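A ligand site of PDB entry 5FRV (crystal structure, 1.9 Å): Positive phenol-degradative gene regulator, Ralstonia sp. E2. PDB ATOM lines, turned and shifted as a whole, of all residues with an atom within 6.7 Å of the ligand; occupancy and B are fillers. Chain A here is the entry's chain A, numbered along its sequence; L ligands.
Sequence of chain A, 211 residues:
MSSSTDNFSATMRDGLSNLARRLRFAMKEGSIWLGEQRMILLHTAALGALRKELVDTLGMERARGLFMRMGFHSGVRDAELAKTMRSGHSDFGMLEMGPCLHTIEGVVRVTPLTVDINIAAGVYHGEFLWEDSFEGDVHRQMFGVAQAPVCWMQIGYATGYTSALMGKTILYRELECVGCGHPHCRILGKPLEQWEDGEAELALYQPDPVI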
ATOM      1  N   LEU A  95     -17.611  -2.647 -10.839  1.00  0.00           N
ATOM      2  CA  LEU A  95     -16.843  -2.071  -9.746  1.00  0.00           C
ATOM      3  C   LEU A  95     -17.790  -1.758  -8.614  1.00  0.00           C
ATOM      4  O   LEU A  95     -17.497  -2.037  -7.449  1.00  0.00           O
ATOM      5  CB  LEU A  95     -16.108  -0.806 -10.217  1.00  0.00           C
ATOM      6  CG  LEU A  95     -15.114  -0.094  -9.288  1.00  0.00           C
ATOM      7  CD1 LEU A  95     -15.817   0.806  -8.278  1.00  0.00           C
ATOM      8  CD2 LEU A  95     -14.189  -1.103  -8.597  1.00  0.00           C
ATOM      9  N   GLU A  96     -18.954  -1.205  -8.969  1.00  0.00           N
ATOM     10  CA  GLU A  96     -19.914  -0.700  -8.004  1.00  0.00           C
ATOM     11  C   GLU A  96     -20.504  -1.759  -7.101  1.00  0.00           C
ATOM     12  O   GLU A  96     -21.005  -1.434  -6.031  1.00  0.00           O
ATOM     13  CB  GLU A  96     -21.074   0.012  -8.717  1.00  0.00           C
ATOM     14  CG  GLU A  96     -20.869   1.502  -8.870  1.00  0.00           C
ATOM     15  CD  GLU A  96     -22.120   2.312  -8.532  1.00  0.00           C
ATOM     16  OE1 GLU A  96     -23.199   1.705  -8.345  1.00  0.00           O
ATOM     17  OE2 GLU A  96     -22.028   3.551  -8.459  1.00  0.00           O
ATOM     18  N   MET A  97     -20.475  -3.008  -7.530  1.00  0.00           N
ATOM     19  CA  MET A  97     -21.024  -4.078  -6.719  1.00  0.00           C
ATOM     20  C   MET A  97     -20.239  -4.225  -5.409  1.00  0.00           C
ATOM     21  O   MET A  97     -20.788  -4.613  -4.391  1.00  0.00           O
ATOM     22  CB  MET A  97     -21.027  -5.377  -7.519  1.00  0.00           C
ATOM     23  CG  MET A  97     -21.996  -5.337  -8.691  1.00  0.00           C
ATOM     24  SD  MET A  97     -22.132  -6.919  -9.556  1.00  0.00           S
ATOM     25  CE  MET A  97     -23.558  -6.619 -10.600  1.00  0.00           C
ATOM     26  N   GLY A  98     -18.949  -3.886  -5.450  1.00  0.00           N
ATOM     27  CA  GLY A  98     -18.113  -3.880  -4.268  1.00  0.00           C
ATOM     28  C   GLY A  98     -18.656  -2.993  -3.169  1.00  0.00           C
ATOM     29  O   GLY A  98     -18.946  -3.464  -2.067  1.00  0.00           O
ATOM     30  N   PRO A  99     -18.784  -1.690  -3.446  1.00  0.00           N
ATOM     31  CA  PRO A  99     -19.375  -0.768  -2.473  1.00  0.00           C
ATOM     32  C   PRO A  99     -20.778  -1.215  -2.048  1.00  0.00           C
ATOM     33  O   PRO A  99     -21.148  -1.072  -0.879  1.00  0.00           O
ATOM     34  CB  PRO A  99     -19.419   0.569  -3.227  1.00  0.00           C
ATOM     35  CG  PRO A  99     -18.250   0.504  -4.151  1.00  0.00           C
ATOM     36  CD  PRO A  99     -18.156  -0.970  -4.581  1.00  0.00           C
ATOM     37  N   CYS A 100     -21.552  -1.780  -2.975  1.00  0.00           N
ATOM     38  CA  CYS A 100     -22.855  -2.316  -2.649  1.00  0.00           C
ATOM     39  C   CYS A 100     -22.774  -3.479  -1.656  1.00  0.00           C
ATOM     40  O   CYS A 100     -23.533  -3.517  -0.686  1.00  0.00           O
ATOM     41  CB  CYS A 100     -23.577  -2.768  -3.929  1.00  0.00           C
ATOM     42  SG  CYS A 100     -24.172  -1.369  -4.966  1.00  0.00           S
ATOM     43  N   HIS A 102     -20.281  -4.333   0.439  1.00  0.00           N
ATOM     44  CA  HIS A 102     -19.825  -3.797   1.679  1.00  0.00           C
ATOM     45  C   HIS A 102     -20.923  -3.191   2.542  1.00  0.00           C
ATOM     46  O   HIS A 102     -20.906  -3.321   3.722  1.00  0.00           O
ATOM     47  CB  HIS A 102     -18.738  -2.767   1.471  1.00  0.00           C
ATOM     48  CG  HIS A 102     -17.513  -3.061   2.239  1.00  0.00           C
ATOM     49  ND1 HIS A 102     -16.368  -2.339   2.127  1.00  0.00           N
ATOM     50  CD2 HIS A 102     -17.241  -4.048   3.112  1.00  0.00           C
ATOM     51  CE1 HIS A 102     -15.445  -2.861   2.887  1.00  0.00           C
ATOM     52  NE2 HIS A 102     -15.945  -3.901   3.504  1.00  0.00           N
ATOM     53  N   THR A 103     -21.842  -2.536   1.896  1.00  0.00           N
ATOM     54  CA  THR A 103     -23.002  -1.921   2.554  1.00  0.00           C
ATOM     55  C   THR A 103     -24.053  -2.943   3.008  1.00  0.00           C
ATOM     56  O   THR A 103     -24.532  -2.873   4.140  1.00  0.00           O
ATOM     57  CB  THR A 103     -23.676  -0.875   1.626  1.00  0.00           C
ATOM     58  OG1 THR A 103     -22.705   0.085   1.202  1.00  0.00           O
ATOM     59  CG2 THR A 103     -24.786  -0.140   2.347  1.00  0.00           C
ATOM     60  N   VAL A 107     -21.001  -3.326   6.919  1.00  0.00           N
ATOM     61  CA  VAL A 107     -19.652  -2.966   7.322  1.00  0.00           C
ATOM     62  C   VAL A 107     -19.501  -1.431   7.344  1.00  0.00           C
ATOM     63  O   VAL A 107     -18.903  -0.858   8.270  1.00  0.00           O
ATOM     64  CB  VAL A 107     -18.630  -3.665   6.373  1.00  0.00           C
ATOM     65  CG1 VAL A 107     -17.224  -3.131   6.526  1.00  0.00           C
ATOM     66  CG2 VAL A 107     -18.670  -5.202   6.613  1.00  0.00           C
ATOM     67  N   VAL A 108     -20.087  -0.782   6.352  1.00  0.00           N
ATOM     68  CA  VAL A 108     -19.909   0.654   6.128  1.00  0.00           C
ATOM     69  C   VAL A 108     -20.873   1.077   5.025  1.00  0.00           C
ATOM     70  O   VAL A 108     -21.303   0.260   4.211  1.00  0.00           O
ATOM     71  CB  VAL A 108     -18.425   1.016   5.750  1.00  0.00           C
ATOM     72  CG1 VAL A 108     -17.973   0.291   4.473  1.00  0.00           C
ATOM     73  CG2 VAL A 108     -18.230   2.541   5.571  1.00  0.00           C
ATOM     74  N   VAL A 110     -21.008   3.076   1.712  1.00  0.00           N
ATOM     75  CA  VAL A 110     -19.991   3.479   0.758  1.00  0.00           C
ATOM     76  C   VAL A 110     -20.601   4.374  -0.297  1.00  0.00           C
ATOM     77  O   VAL A 110     -21.665   4.082  -0.834  1.00  0.00           O
ATOM     78  CB  VAL A 110     -19.354   2.262   0.092  1.00  0.00           C
ATOM     79  CG1 VAL A 110     -18.124   2.687  -0.744  1.00  0.00           C
ATOM     80  CG2 VAL A 110     -18.970   1.243   1.146  1.00  0.00           C
ATOM     81  N   TYR A 124      -6.863   1.898 -13.216  1.00  0.00           N
ATOM     82  CA  TYR A 124      -7.792   2.102 -12.114  1.00  0.00           C
ATOM     83  C   TYR A 124      -7.388   3.279 -11.248  1.00  0.00           C
ATOM     84  O   TYR A 124      -6.270   3.359 -10.744  1.00  0.00           O
ATOM     85  CB  TYR A 124      -7.922   0.864 -11.228  1.00  0.00           C
ATOM     86  CG  TYR A 124      -8.961   1.057 -10.138  1.00  0.00           C
ATOM     87  CD1 TYR A 124     -10.311   0.956 -10.441  1.00  0.00           C
ATOM     88  CD2 TYR A 124      -8.598   1.380  -8.837  1.00  0.00           C
ATOM     89  CE1 TYR A 124     -11.274   1.150  -9.471  1.00  0.00           C
ATOM     90  CE2 TYR A 124      -9.559   1.573  -7.853  1.00  0.00           C
ATOM     91  CZ  TYR A 124     -10.892   1.468  -8.180  1.00  0.00           C
ATOM     92  OH  TYR A 124     -11.862   1.654  -7.238  1.00  0.00           O
ATOM     93  N   PHE A 128     -13.390   6.959  -2.655  1.00  0.00           N
ATOM     94  CA  PHE A 128     -14.687   6.627  -2.054  1.00  0.00           C
ATOM     95  C   PHE A 128     -14.877   7.278  -0.693  1.00  0.00           C
ATOM     96  O   PHE A 128     -13.912   7.450   0.069  1.00  0.00           O
ATOM     97  CB  PHE A 128     -14.836   5.110  -1.882  1.00  0.00           C
ATOM     98  CG  PHE A 128     -14.629   4.329  -3.160  1.00  0.00           C
ATOM     99  CD1 PHE A 128     -13.362   4.056  -3.608  1.00  0.00           C
ATOM    100  CD2 PHE A 128     -15.706   3.855  -3.869  1.00  0.00           C
ATOM    101  CE1 PHE A 128     -13.159   3.358  -4.781  1.00  0.00           C
ATOM    102  CE2 PHE A 128     -15.514   3.150  -5.048  1.00  0.00           C
ATOM    103  CZ  PHE A 128     -14.246   2.897  -5.488  1.00  0.00           C
ATOM    104  N   LEU A 129     -16.132   7.612  -0.393  1.00  0.00           N
ATOM    105  CA  LEU A 129     -16.575   8.043   0.931  1.00  0.00           C
ATOM    106  C   LEU A 129     -17.098   6.851   1.746  1.00  0.00           C
ATOM    107  O   LEU A 129     -17.835   6.002   1.228  1.00  0.00           O
ATOM    108  CB  LEU A 129     -17.671   9.104   0.815  1.00  0.00           C
ATOM    109  CG  LEU A 129     -18.242   9.612   2.135  1.00  0.00           C
ATOM    110  CD1 LEU A 129     -17.203  10.469   2.885  1.00  0.00           C
ATOM    111  CD2 LEU A 129     -19.538  10.398   1.942  1.00  0.00           C
ATOM    112  N   TRP A 130     -16.704   6.823   3.008  1.00  0.00           N
ATOM    113  CA  TRP A 130     -17.157   5.819   3.972  1.00  0.00           C
ATOM    114  C   TRP A 130     -17.921   6.454   5.135  1.00  0.00           C
ATOM    115  O   TRP A 130     -17.307   7.106   5.984  1.00  0.00           O
ATOM    116  CB  TRP A 130     -15.959   5.047   4.525  1.00  0.00           C
ATOM    117  CG  TRP A 130     -15.485   3.876   3.701  1.00  0.00           C
ATOM    118  CD1 TRP A 130     -16.109   3.333   2.616  1.00  0.00           C
ATOM    119  CD2 TRP A 130     -14.291   3.118   3.904  1.00  0.00           C
ATOM    120  NE1 TRP A 130     -15.361   2.269   2.135  1.00  0.00           N
ATOM    121  CE2 TRP A 130     -14.244   2.119   2.913  1.00  0.00           C
ATOM    122  CE3 TRP A 130     -13.255   3.165   4.849  1.00  0.00           C
ATOM    123  CZ2 TRP A 130     -13.211   1.191   2.838  1.00  0.00           C
ATOM    124  CZ3 TRP A 130     -12.207   2.254   4.744  1.00  0.00           C
ATOM    125  CH2 TRP A 130     -12.206   1.278   3.754  1.00  0.00           C
ATOM    126  N   GLN A 154     -11.754  -3.107   6.490  1.00  0.00           N
ATOM    127  CA  GLN A 154     -12.510  -2.431   5.461  1.00  0.00           C
ATOM    128  C   GLN A 154     -11.596  -2.122   4.267  1.00  0.00           C
ATOM    129  O   GLN A 154     -11.982  -2.295   3.107  1.00  0.00           O
ATOM    130  CB  GLN A 154     -13.180  -1.162   6.020  1.00  0.00           C
ATOM    131  CG  GLN A 154     -14.193  -1.474   7.122  1.00  0.00           C
ATOM    132  CD  GLN A 154     -14.932  -0.248   7.653  1.00  0.00           C
ATOM    133  OE1 GLN A 154     -15.618  -0.328   8.681  1.00  0.00           O
ATOM    134  NE2 GLN A 154     -14.830   0.872   6.930  1.00  0.00           N
ATOM    135  N   TYR A 157     -10.687  -5.280   2.309  1.00  0.00           N
ATOM    136  CA  TYR A 157     -11.800  -5.659   1.445  1.00  0.00           C
ATOM    137  C   TYR A 157     -11.719  -4.901   0.133  1.00  0.00           C
ATOM    138  O   TYR A 157     -11.795  -5.502  -0.955  1.00  0.00           O
ATOM    139  CB  TYR A 157     -13.141  -5.410   2.155  1.00  0.00           C
ATOM    140  CG  TYR A 157     -14.364  -5.811   1.343  1.00  0.00           C
ATOM    141  CD1 TYR A 157     -14.805  -5.025   0.278  1.00  0.00           C
ATOM    142  CD2 TYR A 157     -15.074  -6.977   1.629  1.00  0.00           C
ATOM    143  CE1 TYR A 157     -15.901  -5.379  -0.479  1.00  0.00           C
ATOM    144  CE2 TYR A 157     -16.188  -7.346   0.873  1.00  0.00           C
ATOM    145  CZ  TYR A 157     -16.591  -6.540  -0.168  1.00  0.00           C
ATOM    146  OH  TYR A 157     -17.701  -6.890  -0.887  1.00  0.00           O
ATOM    147  N   ALA A 158     -11.572  -3.583   0.230  1.00  0.00           N
ATOM    148  CA  ALA A 158     -11.487  -2.755  -0.958  1.00  0.00           C
ATOM    149  C   ALA A 158     -10.333  -3.231  -1.830  1.00  0.00           C
ATOM    150  O   ALA A 158     -10.474  -3.367  -3.048  1.00  0.00           O
ATOM    151  CB  ALA A 158     -11.318  -1.270  -0.569  1.00  0.00           C
ATOM    152  N   THR A 159      -9.200  -3.530  -1.199  1.00  0.00           N
ATOM    153  CA  THR A 159      -8.004  -3.998  -1.933  1.00  0.00           C
ATOM    154  C   THR A 159      -8.241  -5.358  -2.613  1.00  0.00           C
ATOM    155  O   THR A 159      -7.950  -5.540  -3.794  1.00  0.00           O
ATOM    156  CB  THR A 159      -6.819  -4.096  -0.970  1.00  0.00           C
ATOM    157  OG1 THR A 159      -6.599  -2.814  -0.349  1.00  0.00           O
ATOM    158  CG2 THR A 159      -5.585  -4.524  -1.673  1.00  0.00           C
ATOM    159  N   TYR A 161     -11.221  -6.946  -3.235  1.00  0.00           N
ATOM    160  CA  TYR A 161     -12.268  -6.885  -4.244  1.00  0.00           C
ATOM    161  C   TYR A 161     -11.725  -6.306  -5.559  1.00  0.00           C
ATOM    162  O   TYR A 161     -11.839  -6.918  -6.635  1.00  0.00           O
ATOM    163  CB  TYR A 161     -13.461  -6.052  -3.734  1.00  0.00           C
ATOM    164  CG  TYR A 161     -14.599  -5.997  -4.743  1.00  0.00           C
ATOM    165  CD1 TYR A 161     -14.604  -5.052  -5.767  1.00  0.00           C
ATOM    166  CD2 TYR A 161     -15.638  -6.914  -4.694  1.00  0.00           C
ATOM    167  CE1 TYR A 161     -15.603  -5.016  -6.713  1.00  0.00           C
ATOM    168  CE2 TYR A 161     -16.661  -6.861  -5.635  1.00  0.00           C
ATOM    169  CZ  TYR A 161     -16.639  -5.913  -6.642  1.00  0.00           C
ATOM    170  OH  TYR A 161     -17.639  -5.856  -7.579  1.00  0.00           O
ATOM    171  N   THR A 162     -11.127  -5.124  -5.483  1.00  0.00           N
ATOM    172  CA  THR A 162     -10.699  -4.452  -6.711  1.00  0.00           C
ATOM    173  C   THR A 162      -9.616  -5.211  -7.422  1.00  0.00           C
ATOM    174  O   THR A 162      -9.621  -5.301  -8.651  1.00  0.00           O
ATOM    175  CB  THR A 162     -10.218  -3.052  -6.411  1.00  0.00           C
ATOM    176  OG1 THR A 162     -11.157  -2.417  -5.528  1.00  0.00           O
ATOM    177  CG2 THR A 162     -10.098  -2.263  -7.714  1.00  0.00           C
ATOM    178  N   TYR A 172      -5.358   0.112  -1.534  1.00  0.00           N
ATOM    179  CA  TYR A 172      -6.071   1.290  -0.988  1.00  0.00           C
ATOM    180  C   TYR A 172      -5.470   1.816   0.293  1.00  0.00           C
ATOM    181  O   TYR A 172      -4.839   1.095   1.060  1.00  0.00           O
ATOM    182  CB  TYR A 172      -7.542   0.987  -0.674  1.00  0.00           C
ATOM    183  CG  TYR A 172      -8.430   0.798  -1.871  1.00  0.00           C
ATOM    184  CD1 TYR A 172      -8.335  -0.341  -2.656  1.00  0.00           C
ATOM    185  CD2 TYR A 172      -9.402   1.734  -2.186  1.00  0.00           C
ATOM    186  CE1 TYR A 172      -9.144  -0.522  -3.750  1.00  0.00           C
ATOM    187  CE2 TYR A 172     -10.238   1.550  -3.262  1.00  0.00           C
ATOM    188  CZ  TYR A 172     -10.099   0.399  -4.039  1.00  0.00           C
ATOM    189  OH  TYR A 172     -10.922   0.191  -5.126  1.00  0.00           O
ATOM    190  N   ILE A 187     -11.191   7.124   1.167  1.00  0.00           N
ATOM    191  CA  ILE A 187     -10.145   6.227   0.727  1.00  0.00           C
ATOM    192  C   ILE A 187      -9.740   6.472  -0.735  1.00  0.00           C
ATOM    193  O   ILE A 187     -10.478   7.067  -1.527  1.00  0.00           O
ATOM    194  CB  ILE A 187     -10.580   4.737   0.881  1.00  0.00           C
ATOM    195  CG1 ILE A 187     -11.537   4.328  -0.238  1.00  0.00           C
ATOM    196  CG2 ILE A 187     -11.202   4.501   2.277  1.00  0.00           C
ATOM    197  CD1 ILE A 187     -12.039   2.889  -0.165  1.00  0.00           C
HETATM  198  C1  LIG L   1     -14.304  -1.069  -4.671  1.00  0.00           C
HETATM  199  C2  LIG L   1     -14.724  -0.842  -3.232  1.00  0.00           C
HETATM  200  C3  LIG L   1     -15.223  -1.905  -2.487  1.00  0.00           C
HETATM  201  C4  LIG L   1     -15.623  -1.683  -1.180  1.00  0.00           C
HETATM  202  C5  LIG L   1     -14.625   0.422  -2.679  1.00  0.00           C
HETATM  203  C6  LIG L   1     -15.011   0.640  -1.375  1.00  0.00           C
HETATM  204  C7  LIG L   1     -15.517  -0.420  -0.635  1.00  0.00           C
HETATM  205  O1  LIG L   1     -15.912  -0.220   0.691  1.00  0.00           O
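ND1 of His 102 sits at hydrogen-bond distance from O1 of the ligand (2.6 Å).
The indole nitrogen (NE1) of Trp 130 lies within hydrogen-bond range of an oxygen (O1) of the ligand (2.9 Å).
The backbone carbonyl oxygen (O) of His 102 sits at hydrogen-bond distance from the backbone NH (N) of Val 107.
OG1 of Thr 103 sits at hydrogen-bond distance from N of Val 110.
The side-chain hydroxyl (OH) of Tyr 172 is in hydrogen-bond range of the side-chain hydroxyl (OG1) of Thr 162 (2.6 Å).
OG1 of Thr 162 lies within hydrogen-bond range of O of Ala 158, at 2.7 Å.
The side-chain hydroxyl of Tyr 172 is in hydrogen-bond range of the side-chain hydroxyl of Tyr 124 (2.7 Å).
The side-chain hydroxyl (OG1) of Thr 159 sits at hydrogen-bond distance from the backbone NH (N) of Tyr 172.
The side-chain hydroxyl of Thr 103 is in hydrogen-bond range of the backbone carbonyl oxygen of Pro 99, at 2.8 Å.
O of Phe 128 lies within hydrogen-bond range of N of Ile 187, at 3.0 Å.
Leu 95 touches the ligand (CD2 to C1, 3.9 Å).
C of Gly 98 touches C3 of the ligand, 3.7 Å away.
Pro 99 touches the ligand (CD to C2, 3.7 Å).
CG2 of Val 110 touches O1 of the ligand (3.4 Å).
Phe 128 touches the ligand (CE2 to C5, 3.7 Å).
Tyr 157 touches the ligand (CD1 to C4, 3.7 Å).
Thr 162 touches the ligand.
OH of Tyr 172 touches C1 of the ligand (3.6 Å).
Ile 187 touches the ligand.
Hydrophobic or aromatic side chains within 4 Å of the ligand: Leu 95, Pro 99, His 102, Val 110, Phe 128, Trp 130, Tyr 157 and Ile 187.
Of the 23 residues printed, 11 come within 4 Å of the ligand.
The nearest printed residue that does not touch the ligand is Ala 158 (4.1 Å).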
